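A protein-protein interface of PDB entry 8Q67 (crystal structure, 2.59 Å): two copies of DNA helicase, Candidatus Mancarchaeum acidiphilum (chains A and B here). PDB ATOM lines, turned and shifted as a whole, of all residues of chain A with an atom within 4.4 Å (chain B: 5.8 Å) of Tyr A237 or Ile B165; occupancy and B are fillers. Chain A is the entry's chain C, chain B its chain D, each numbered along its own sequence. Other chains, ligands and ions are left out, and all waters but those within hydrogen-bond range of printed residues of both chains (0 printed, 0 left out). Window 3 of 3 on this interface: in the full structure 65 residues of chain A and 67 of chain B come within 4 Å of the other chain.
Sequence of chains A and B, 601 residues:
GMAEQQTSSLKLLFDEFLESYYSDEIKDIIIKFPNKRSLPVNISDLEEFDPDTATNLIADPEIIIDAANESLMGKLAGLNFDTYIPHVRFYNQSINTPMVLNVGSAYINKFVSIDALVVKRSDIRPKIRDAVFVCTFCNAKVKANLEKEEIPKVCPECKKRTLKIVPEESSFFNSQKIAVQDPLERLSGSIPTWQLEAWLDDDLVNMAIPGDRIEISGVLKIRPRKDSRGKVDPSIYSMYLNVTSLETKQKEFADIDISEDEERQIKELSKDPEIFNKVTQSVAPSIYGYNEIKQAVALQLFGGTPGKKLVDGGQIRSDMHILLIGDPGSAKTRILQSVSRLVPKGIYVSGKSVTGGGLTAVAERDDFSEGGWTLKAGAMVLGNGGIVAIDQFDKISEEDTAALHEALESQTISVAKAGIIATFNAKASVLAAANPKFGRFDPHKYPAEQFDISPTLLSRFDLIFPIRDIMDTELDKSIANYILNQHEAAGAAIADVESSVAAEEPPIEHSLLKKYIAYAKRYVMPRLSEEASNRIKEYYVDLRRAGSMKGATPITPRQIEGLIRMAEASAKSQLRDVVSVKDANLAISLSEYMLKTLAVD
The backbone NH (N) of Ile B128 lies within hydrogen-bond range of the backbone carbonyl oxygen (O) of Ser A235 (3.1 Å). The backbone NH (N) of Tyr A237 sits at hydrogen-bond distance from the backbone carbonyl oxygen (O) of Pro B126, at 2.8 Å. The guanidinium group (NH2) of Arg A225 lies close to the guanidinium group (NH2) of Arg B125 (3.1 Å).
N of Arg A225 lies within hydrogen-bond range of O of Ile A236 (3.4 Å).
CG of Pro B126 touches CG2 of Ile A222, 3.8 Å away. Ile A222 touches Phe B172 (CD1 to CZ, 3.3 Å). Ser A235 touches Pro B126. Lys B127 touches Ser A235. Ile A236 touches Pro B126. Ile A236 touches Lys B127 (CG1 to CG, 3.6 Å). CB of Arg B125 touches O of Tyr A237, at 3.6 Å. CG2 of Ile B165 touches OH of Tyr A237 (3.9 Å). CG of Pro B167 touches OH of Tyr A237, 3.2 Å away. Tyr A237 touches Phe B172.
Printed residues of chain B within 4 Å of Ile A222: Pro B126 and Phe B172. Of chain B, only Arg B125, Pro B126, Ile B128, Ile B165, Pro B167 and Phe B172 come within 4 Å of Tyr A237. Of the printed residues of chain A, Ile B128 touches Ser A235 (3.1 Å) and Tyr A237 (3.8 Å). Of the printed residues of chain A, Leu B146 touches Ser A235 (3.2 Å). Ile B165 touches just these residues of chain A: Pro A234 and Tyr A237. Val B166 touches none of the printed residues of chain A. Ser B170 touches none of the printed residues of chain A. The nearest residue of chain B that does not touch Tyr A237 is Lys B127 (4.9 Å).
Printed residues of chain B that touch a printed residue of chain A: Arg B125, Pro B126, Lys B127, Ile B128, Leu B146, Ile B165, Pro B167 and Phe B172. Hydrophobic or aromatic side chains of chain B that line the printed part of chain A: Pro B126, Ile B128, Leu B146, Ile B165, Pro B167 and Phe B172. Of the 9 printed residues of chain A, 6 touch a printed residue of chain B. Along chain A the printed residues that touch a printed residue of chain B span positions 222 to 237. Among the printed residues, 16 pairs touch across the chains. Among the printed residues, no Asp or Glu carboxylate lies within 4 Å of a Lys or Arg side-chain nitrogen of the other chain.
No position is printed for both chains. Of the 16 pairs that touch across the chains among the printed residues, none has its exchanged pair printed and touching as well.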
ATOM      1  N   ILE A 222       4.157 -20.702  -0.418  1.00  0.00           N
ATOM      2  CA  ILE A 222       5.554 -20.412  -0.729  1.00  0.00           C
ATOM      3  C   ILE A 222       6.120 -19.483   0.339  1.00  0.00           C
ATOM      4  O   ILE A 222       5.387 -18.738   0.996  1.00  0.00           O
ATOM      5  CB  ILE A 222       5.718 -19.798  -2.138  1.00  0.00           C
ATOM      6  CG1 ILE A 222       4.665 -18.716  -2.373  1.00  0.00           C
ATOM      7  CG2 ILE A 222       5.599 -20.870  -3.214  1.00  0.00           C
ATOM      8  CD1 ILE A 222       5.019 -17.750  -3.487  1.00  0.00           C
ATOM      9  N   ARG A 223       7.412 -19.658   0.511  1.00  0.00           N
ATOM     10  CA  ARG A 223       8.243 -18.999   1.472  1.00  0.00           C
ATOM     11  C   ARG A 223       9.524 -18.670   0.787  1.00  0.00           C
ATOM     12  O   ARG A 223       9.966 -19.394  -0.070  1.00  0.00           O
ATOM     13  CB  ARG A 223       8.584 -20.007   2.534  1.00  0.00           C
ATOM     14  CG  ARG A 223       8.500 -19.496   3.931  1.00  0.00           C
ATOM     15  CD  ARG A 223       9.233 -20.423   4.866  1.00  0.00           C
ATOM     16  NE  ARG A 223       9.534 -21.724   4.294  1.00  0.00           N
ATOM     17  CZ  ARG A 223       9.056 -22.862   4.770  1.00  0.00           C
ATOM     18  NH1 ARG A 223       8.246 -22.855   5.804  1.00  0.00           N
ATOM     19  NH2 ARG A 223       9.383 -24.006   4.213  1.00  0.00           N
ATOM     20  N   PRO A 224      10.129 -17.561   1.144  1.00  0.00           N
ATOM     21  CA  PRO A 224      11.368 -17.237   0.473  1.00  0.00           C
ATOM     22  C   PRO A 224      12.403 -18.257   0.836  1.00  0.00           C
ATOM     23  O   PRO A 224      12.527 -18.587   1.985  1.00  0.00           O
ATOM     24  CB  PRO A 224      11.707 -15.871   1.028  1.00  0.00           C
ATOM     25  CG  PRO A 224      10.893 -15.726   2.246  1.00  0.00           C
ATOM     26  CD  PRO A 224       9.655 -16.476   1.992  1.00  0.00           C
ATOM     27  N   ARG A 225      13.143 -18.735  -0.144  1.00  0.00           N
ATOM     28  CA  ARG A 225      14.148 -19.742   0.073  1.00  0.00           C
ATOM     29  C   ARG A 225      15.368 -19.230   0.779  1.00  0.00           C
ATOM     30  O   ARG A 225      15.845 -18.164   0.485  1.00  0.00           O
ATOM     31  CB  ARG A 225      14.550 -20.332  -1.261  1.00  0.00           C
ATOM     32  CG  ARG A 225      15.543 -21.470  -1.182  1.00  0.00           C
ATOM     33  CD  ARG A 225      15.169 -22.629  -2.076  1.00  0.00           C
ATOM     34  NE  ARG A 225      16.248 -23.592  -2.134  1.00  0.00           N
ATOM     35  CZ  ARG A 225      17.502 -23.260  -2.374  1.00  0.00           C
ATOM     36  NH1 ARG A 225      17.817 -22.006  -2.592  1.00  0.00           N
ATOM     37  NH2 ARG A 225      18.439 -24.177  -2.391  1.00  0.00           N
ATOM     38  N   PRO A 234      15.489 -13.012  -3.177  1.00  0.00           N
ATOM     39  CA  PRO A 234      14.118 -12.533  -3.281  1.00  0.00           C
ATOM     40  C   PRO A 234      13.432 -12.973  -4.554  1.00  0.00           C
ATOM     41  O   PRO A 234      12.306 -12.564  -4.752  1.00  0.00           O
ATOM     42  CB  PRO A 234      14.272 -11.012  -3.267  1.00  0.00           C
ATOM     43  CG  PRO A 234      15.739 -10.730  -3.238  1.00  0.00           C
ATOM     44  CD  PRO A 234      16.452 -11.991  -3.587  1.00  0.00           C
ATOM     45  N   SER A 235      14.083 -13.772  -5.392  1.00  0.00           N
ATOM     46  CA  SER A 235      13.453 -14.240  -6.610  1.00  0.00           C
ATOM     47  C   SER A 235      13.095 -15.709  -6.477  1.00  0.00           C
ATOM     48  O   SER A 235      12.087 -16.143  -6.995  1.00  0.00           O
ATOM     49  CB  SER A 235      14.367 -14.066  -7.808  1.00  0.00           C
ATOM     50  OG  SER A 235      14.617 -12.712  -8.070  1.00  0.00           O
ATOM     51  N   ILE A 236      13.887 -16.454  -5.723  1.00  0.00           N
ATOM     52  CA  ILE A 236      13.682 -17.874  -5.542  1.00  0.00           C
ATOM     53  C   ILE A 236      12.925 -18.169  -4.269  1.00  0.00           C
ATOM     54  O   ILE A 236      13.155 -17.540  -3.279  1.00  0.00           O
ATOM     55  CB  ILE A 236      15.029 -18.567  -5.606  1.00  0.00           C
ATOM     56  CG1 ILE A 236      15.506 -18.547  -7.037  1.00  0.00           C
ATOM     57  CG2 ILE A 236      14.954 -20.016  -5.215  1.00  0.00           C
ATOM     58  CD1 ILE A 236      16.681 -17.645  -7.275  1.00  0.00           C
ATOM     59  N   TYR A 237      11.985 -19.107  -4.326  1.00  0.00           N
ATOM     60  CA  TYR A 237      11.124 -19.467  -3.213  1.00  0.00           C
ATOM     61  C   TYR A 237      11.058 -20.971  -2.881  1.00  0.00           C
ATOM     62  O   TYR A 237      11.442 -21.799  -3.667  1.00  0.00           O
ATOM     63  CB  TYR A 237       9.723 -18.969  -3.526  1.00  0.00           C
ATOM     64  CG  TYR A 237       9.488 -17.527  -3.224  1.00  0.00           C
ATOM     65  CD1 TYR A 237       9.964 -16.543  -4.037  1.00  0.00           C
ATOM     66  CD2 TYR A 237       8.760 -17.162  -2.148  1.00  0.00           C
ATOM     67  CE1 TYR A 237       9.749 -15.228  -3.756  1.00  0.00           C
ATOM     68  CE2 TYR A 237       8.539 -15.858  -1.851  1.00  0.00           C
ATOM     69  CZ  TYR A 237       9.035 -14.898  -2.666  1.00  0.00           C
ATOM     70  OH  TYR A 237       8.804 -13.596  -2.373  1.00  0.00           O
ATOM     71  N   SER A 238      10.609 -21.299  -1.680  1.00  0.00           N
ATOM     72  CA  SER A 238      10.457 -22.677  -1.219  1.00  0.00           C
ATOM     73  C   SER A 238       8.994 -23.001  -1.086  1.00  0.00           C
ATOM     74  O   SER A 238       8.220 -22.133  -0.971  1.00  0.00           O
ATOM     75  CB  SER A 238      11.098 -22.844   0.131  1.00  0.00           C
ATOM     76  OG  SER A 238      12.472 -23.059  -0.008  1.00  0.00           O
ATOM     77  N   ILE B 124      11.907 -28.817  -6.856  1.00  0.00           N
ATOM     78  CA  ILE B 124      11.347 -27.723  -7.638  1.00  0.00           C
ATOM     79  C   ILE B 124      11.267 -26.485  -6.755  1.00  0.00           C
ATOM     80  O   ILE B 124      10.770 -26.542  -5.623  1.00  0.00           O
ATOM     81  CB  ILE B 124       9.970 -28.100  -8.204  1.00  0.00           C
ATOM     82  CG1 ILE B 124      10.083 -29.321  -9.121  1.00  0.00           C
ATOM     83  CG2 ILE B 124       9.369 -26.925  -8.958  1.00  0.00           C
ATOM     84  CD1 ILE B 124       8.776 -29.723  -9.777  1.00  0.00           C
ATOM     85  N   ARG B 125      11.685 -25.358  -7.288  1.00  0.00           N
ATOM     86  CA  ARG B 125      11.639 -24.128  -6.555  1.00  0.00           C
ATOM     87  C   ARG B 125      10.998 -23.052  -7.362  1.00  0.00           C
ATOM     88  O   ARG B 125      11.533 -22.654  -8.358  1.00  0.00           O
ATOM     89  CB  ARG B 125      13.048 -23.680  -6.264  1.00  0.00           C
ATOM     90  CG  ARG B 125      13.896 -24.702  -5.556  1.00  0.00           C
ATOM     91  CD  ARG B 125      15.342 -24.551  -5.939  1.00  0.00           C
ATOM     92  NE  ARG B 125      16.176 -25.521  -5.267  1.00  0.00           N
ATOM     93  CZ  ARG B 125      17.491 -25.452  -5.217  1.00  0.00           C
ATOM     94  NH1 ARG B 125      18.117 -24.446  -5.777  1.00  0.00           N
ATOM     95  NH2 ARG B 125      18.175 -26.374  -4.578  1.00  0.00           N
ATOM     96  N   PRO B 126       9.870 -22.514  -6.905  1.00  0.00           N
ATOM     97  CA  PRO B 126       9.220 -21.409  -7.630  1.00  0.00           C
ATOM     98  C   PRO B 126      10.155 -20.210  -7.745  1.00  0.00           C
ATOM     99  O   PRO B 126      10.934 -19.914  -6.837  1.00  0.00           O
ATOM    100  CB  PRO B 126       7.994 -21.086  -6.762  1.00  0.00           C
ATOM    101  CG  PRO B 126       7.704 -22.403  -6.023  1.00  0.00           C
ATOM    102  CD  PRO B 126       9.099 -22.909  -5.709  1.00  0.00           C
ATOM    103  N   LYS B 127      10.116 -19.541  -8.886  1.00  0.00           N
ATOM    104  CA  LYS B 127      10.956 -18.390  -9.155  1.00  0.00           C
ATOM    105  C   LYS B 127      10.120 -17.346  -9.838  1.00  0.00           C
ATOM    106  O   LYS B 127       9.370 -17.666 -10.699  1.00  0.00           O
ATOM    107  CB  LYS B 127      12.074 -18.791 -10.086  1.00  0.00           C
ATOM    108  CG  LYS B 127      13.348 -18.013  -9.902  1.00  0.00           C
ATOM    109  CD  LYS B 127      14.389 -18.459 -10.906  1.00  0.00           C
ATOM    110  CE  LYS B 127      15.553 -17.495 -11.008  1.00  0.00           C
ATOM    111  NZ  LYS B 127      16.531 -17.929 -12.034  1.00  0.00           N
ATOM    112  N   ILE B 128      10.272 -16.090  -9.462  1.00  0.00           N
ATOM    113  CA  ILE B 128       9.489 -15.008 -10.020  1.00  0.00           C
ATOM    114  C   ILE B 128       9.934 -14.487 -11.344  1.00  0.00           C
ATOM    115  O   ILE B 128      11.093 -14.270 -11.541  1.00  0.00           O
ATOM    116  CB  ILE B 128       9.552 -13.823  -9.095  1.00  0.00           C
ATOM    117  CG1 ILE B 128       9.382 -14.287  -7.675  1.00  0.00           C
ATOM    118  CG2 ILE B 128       8.442 -12.866  -9.390  1.00  0.00           C
ATOM    119  CD1 ILE B 128       8.709 -13.270  -6.797  1.00  0.00           C
ATOM    120  N   ALA B 131       7.580  -9.437 -11.680  1.00  0.00           N
ATOM    121  CA  ALA B 131       7.448  -9.073 -10.307  1.00  0.00           C
ATOM    122  C   ALA B 131       6.745  -7.784 -10.119  1.00  0.00           C
ATOM    123  O   ALA B 131       6.780  -6.929 -10.957  1.00  0.00           O
ATOM    124  CB  ALA B 131       8.815  -8.970  -9.704  1.00  0.00           C
ATOM    125  N   VAL B 132       6.089  -7.675  -8.990  1.00  0.00           N
ATOM    126  CA  VAL B 132       5.400  -6.467  -8.554  1.00  0.00           C
ATOM    127  C   VAL B 132       5.974  -6.067  -7.196  1.00  0.00           C
ATOM    128  O   VAL B 132       6.079  -6.903  -6.292  1.00  0.00           O
ATOM    129  CB  VAL B 132       3.877  -6.691  -8.470  1.00  0.00           C
ATOM    130  CG1 VAL B 132       3.209  -5.571  -7.689  1.00  0.00           C
ATOM    131  CG2 VAL B 132       3.274  -6.823  -9.868  1.00  0.00           C
ATOM    132  N   PHE B 133       6.366  -4.800  -7.066  1.00  0.00           N
ATOM    133  CA  PHE B 133       6.887  -4.242  -5.827  1.00  0.00           C
ATOM    134  C   PHE B 133       5.974  -3.110  -5.376  1.00  0.00           C
ATOM    135  O   PHE B 133       5.404  -2.396  -6.203  1.00  0.00           O
ATOM    136  CB  PHE B 133       8.318  -3.708  -6.004  1.00  0.00           C
ATOM    137  CG  PHE B 133       9.295  -4.741  -6.490  1.00  0.00           C
ATOM    138  CD1 PHE B 133       9.436  -4.994  -7.845  1.00  0.00           C
ATOM    139  CD2 PHE B 133      10.075  -5.453  -5.594  1.00  0.00           C
ATOM    140  CE1 PHE B 133      10.329  -5.943  -8.294  1.00  0.00           C
ATOM    141  CE2 PHE B 133      10.969  -6.402  -6.039  1.00  0.00           C
ATOM    142  CZ  PHE B 133      11.098  -6.644  -7.391  1.00  0.00           C
ATOM    143  N   VAL B 134       5.841  -2.947  -4.060  1.00  0.00           N
ATOM    144  CA  VAL B 134       5.047  -1.872  -3.476  1.00  0.00           C
ATOM    145  C   VAL B 134       5.916  -1.086  -2.500  1.00  0.00           C
ATOM    146  O   VAL B 134       6.685  -1.671  -1.728  1.00  0.00           O
ATOM    147  CB  VAL B 134       3.786  -2.407  -2.769  1.00  0.00           C
ATOM    148  CG1 VAL B 134       3.220  -1.344  -1.837  1.00  0.00           C
ATOM    149  CG2 VAL B 134       2.760  -2.855  -3.792  1.00  0.00           C
ATOM    150  N   LEU B 146      12.109  -9.890 -13.740  1.00  0.00           N
ATOM    151  CA  LEU B 146      13.349 -10.278 -13.128  1.00  0.00           C
ATOM    152  C   LEU B 146      14.333 -10.970 -14.027  1.00  0.00           C
ATOM    153  O   LEU B 146      15.513 -10.940 -13.760  1.00  0.00           O
ATOM    154  CB  LEU B 146      13.086 -11.083 -11.888  1.00  0.00           C
ATOM    155  CG  LEU B 146      12.282 -10.265 -10.908  1.00  0.00           C
ATOM    156  CD1 LEU B 146      12.579 -10.717  -9.512  1.00  0.00           C
ATOM    157  CD2 LEU B 146      12.634  -8.816 -11.053  1.00  0.00           C
ATOM    158  N   LEU B 163      11.019  -0.302  -1.340  1.00  0.00           N
ATOM    159  CA  LEU B 163      10.238  -1.209  -2.166  1.00  0.00           C
ATOM    160  C   LEU B 163      10.275  -2.619  -1.591  1.00  0.00           C
ATOM    161  O   LEU B 163      11.331  -3.118  -1.187  1.00  0.00           O
ATOM    162  CB  LEU B 163      10.773  -1.208  -3.596  1.00  0.00           C
ATOM    163  CG  LEU B 163      10.478   0.015  -4.468  1.00  0.00           C
ATOM    164  CD1 LEU B 163      11.099  -0.197  -5.847  1.00  0.00           C
ATOM    165  CD2 LEU B 163       8.990   0.282  -4.586  1.00  0.00           C
ATOM    166  N   LYS B 164       9.108  -3.266  -1.575  1.00  0.00           N
ATOM    167  CA  LYS B 164       8.926  -4.599  -1.019  1.00  0.00           C
ATOM    168  C   LYS B 164       8.184  -5.450  -2.035  1.00  0.00           C
ATOM    169  O   LYS B 164       7.135  -5.041  -2.542  1.00  0.00           O
ATOM    170  CB  LYS B 164       8.151  -4.519   0.300  1.00  0.00           C
ATOM    171  CG  LYS B 164       7.669  -5.837   0.869  1.00  0.00           C
ATOM    172  CD  LYS B 164       6.878  -5.597   2.157  1.00  0.00           C
ATOM    173  CE  LYS B 164       5.485  -5.045   1.880  1.00  0.00           C
ATOM    174  NZ  LYS B 164       4.583  -5.123   3.071  1.00  0.00           N
ATOM    175  N   ILE B 165       8.730  -6.625  -2.337  1.00  0.00           N
ATOM    176  CA  ILE B 165       8.096  -7.500  -3.309  1.00  0.00           C
ATOM    177  C   ILE B 165       6.811  -8.069  -2.716  1.00  0.00           C
ATOM    178  O   ILE B 165       6.752  -8.437  -1.534  1.00  0.00           O
ATOM    179  CB  ILE B 165       9.058  -8.620  -3.736  1.00  0.00           C
ATOM    180  CG1 ILE B 165       8.672  -9.137  -5.122  1.00  0.00           C
ATOM    181  CG2 ILE B 165       9.029  -9.754  -2.712  1.00  0.00           C
ATOM    182  CD1 ILE B 165       9.778  -9.872  -5.828  1.00  0.00           C
ATOM    183  N   VAL B 166       5.773  -8.133  -3.540  1.00  0.00           N
ATOM    184  CA  VAL B 166       4.476  -8.687  -3.163  1.00  0.00           C
ATOM    185  C   VAL B 166       4.257  -9.977  -3.947  1.00  0.00           C
ATOM    186  O   VAL B 166       3.801  -9.954  -5.098  1.00  0.00           O
ATOM    187  CB  VAL B 166       3.375  -7.642  -3.382  1.00  0.00           C
ATOM    188  CG1 VAL B 166       3.385  -7.186  -4.811  1.00  0.00           C
ATOM    189  CG2 VAL B 166       2.028  -8.228  -3.045  1.00  0.00           C
ATOM    190  N   PRO B 167       4.572 -11.129  -3.352  1.00  0.00           N
ATOM    191  CA  PRO B 167       4.502 -12.387  -4.112  1.00  0.00           C
ATOM    192  C   PRO B 167       3.112 -12.692  -4.645  1.00  0.00           C
ATOM    193  O   PRO B 167       2.983 -13.331  -5.698  1.00  0.00           O
ATOM    194  CB  PRO B 167       4.964 -13.434  -3.084  1.00  0.00           C
ATOM    195  CG  PRO B 167       5.741 -12.631  -2.025  1.00  0.00           C
ATOM    196  CD  PRO B 167       4.972 -11.347  -1.951  1.00  0.00           C
ATOM    197  N   SER B 170       2.900 -11.185  -7.999  1.00  0.00           N
ATOM    198  CA  SER B 170       3.977 -11.541  -8.907  1.00  0.00           C
ATOM    199  C   SER B 170       3.685 -12.887  -9.562  1.00  0.00           C
ATOM    200  O   SER B 170       2.939 -13.713  -9.031  1.00  0.00           O
ATOM    201  CB  SER B 170       5.303 -11.598  -8.152  1.00  0.00           C
ATOM    202  OG  SER B 170       5.423 -10.485  -7.281  1.00  0.00           O
ATOM    203  N   PHE B 172       5.158 -16.566 -11.200  1.00  0.00           N
ATOM    204  CA  PHE B 172       6.172 -17.558 -10.862  1.00  0.00           C
ATOM    205  C   PHE B 172       6.309 -18.568 -12.001  1.00  0.00           C
ATOM    206  O   PHE B 172       5.384 -18.777 -12.790  1.00  0.00           O
ATOM    207  CB  PHE B 172       5.817 -18.300  -9.551  1.00  0.00           C
ATOM    208  CG  PHE B 172       5.997 -17.471  -8.301  1.00  0.00           C
ATOM    209  CD1 PHE B 172       5.021 -16.570  -7.902  1.00  0.00           C
ATOM    210  CD2 PHE B 172       7.130 -17.611  -7.516  1.00  0.00           C
ATOM    211  CE1 PHE B 172       5.181 -15.807  -6.758  1.00  0.00           C
ATOM    212  CE2 PHE B 172       7.292 -16.859  -6.365  1.00  0.00           C
ATOM    213  CZ  PHE B 172       6.319 -15.953  -5.989  1.00  0.00           C
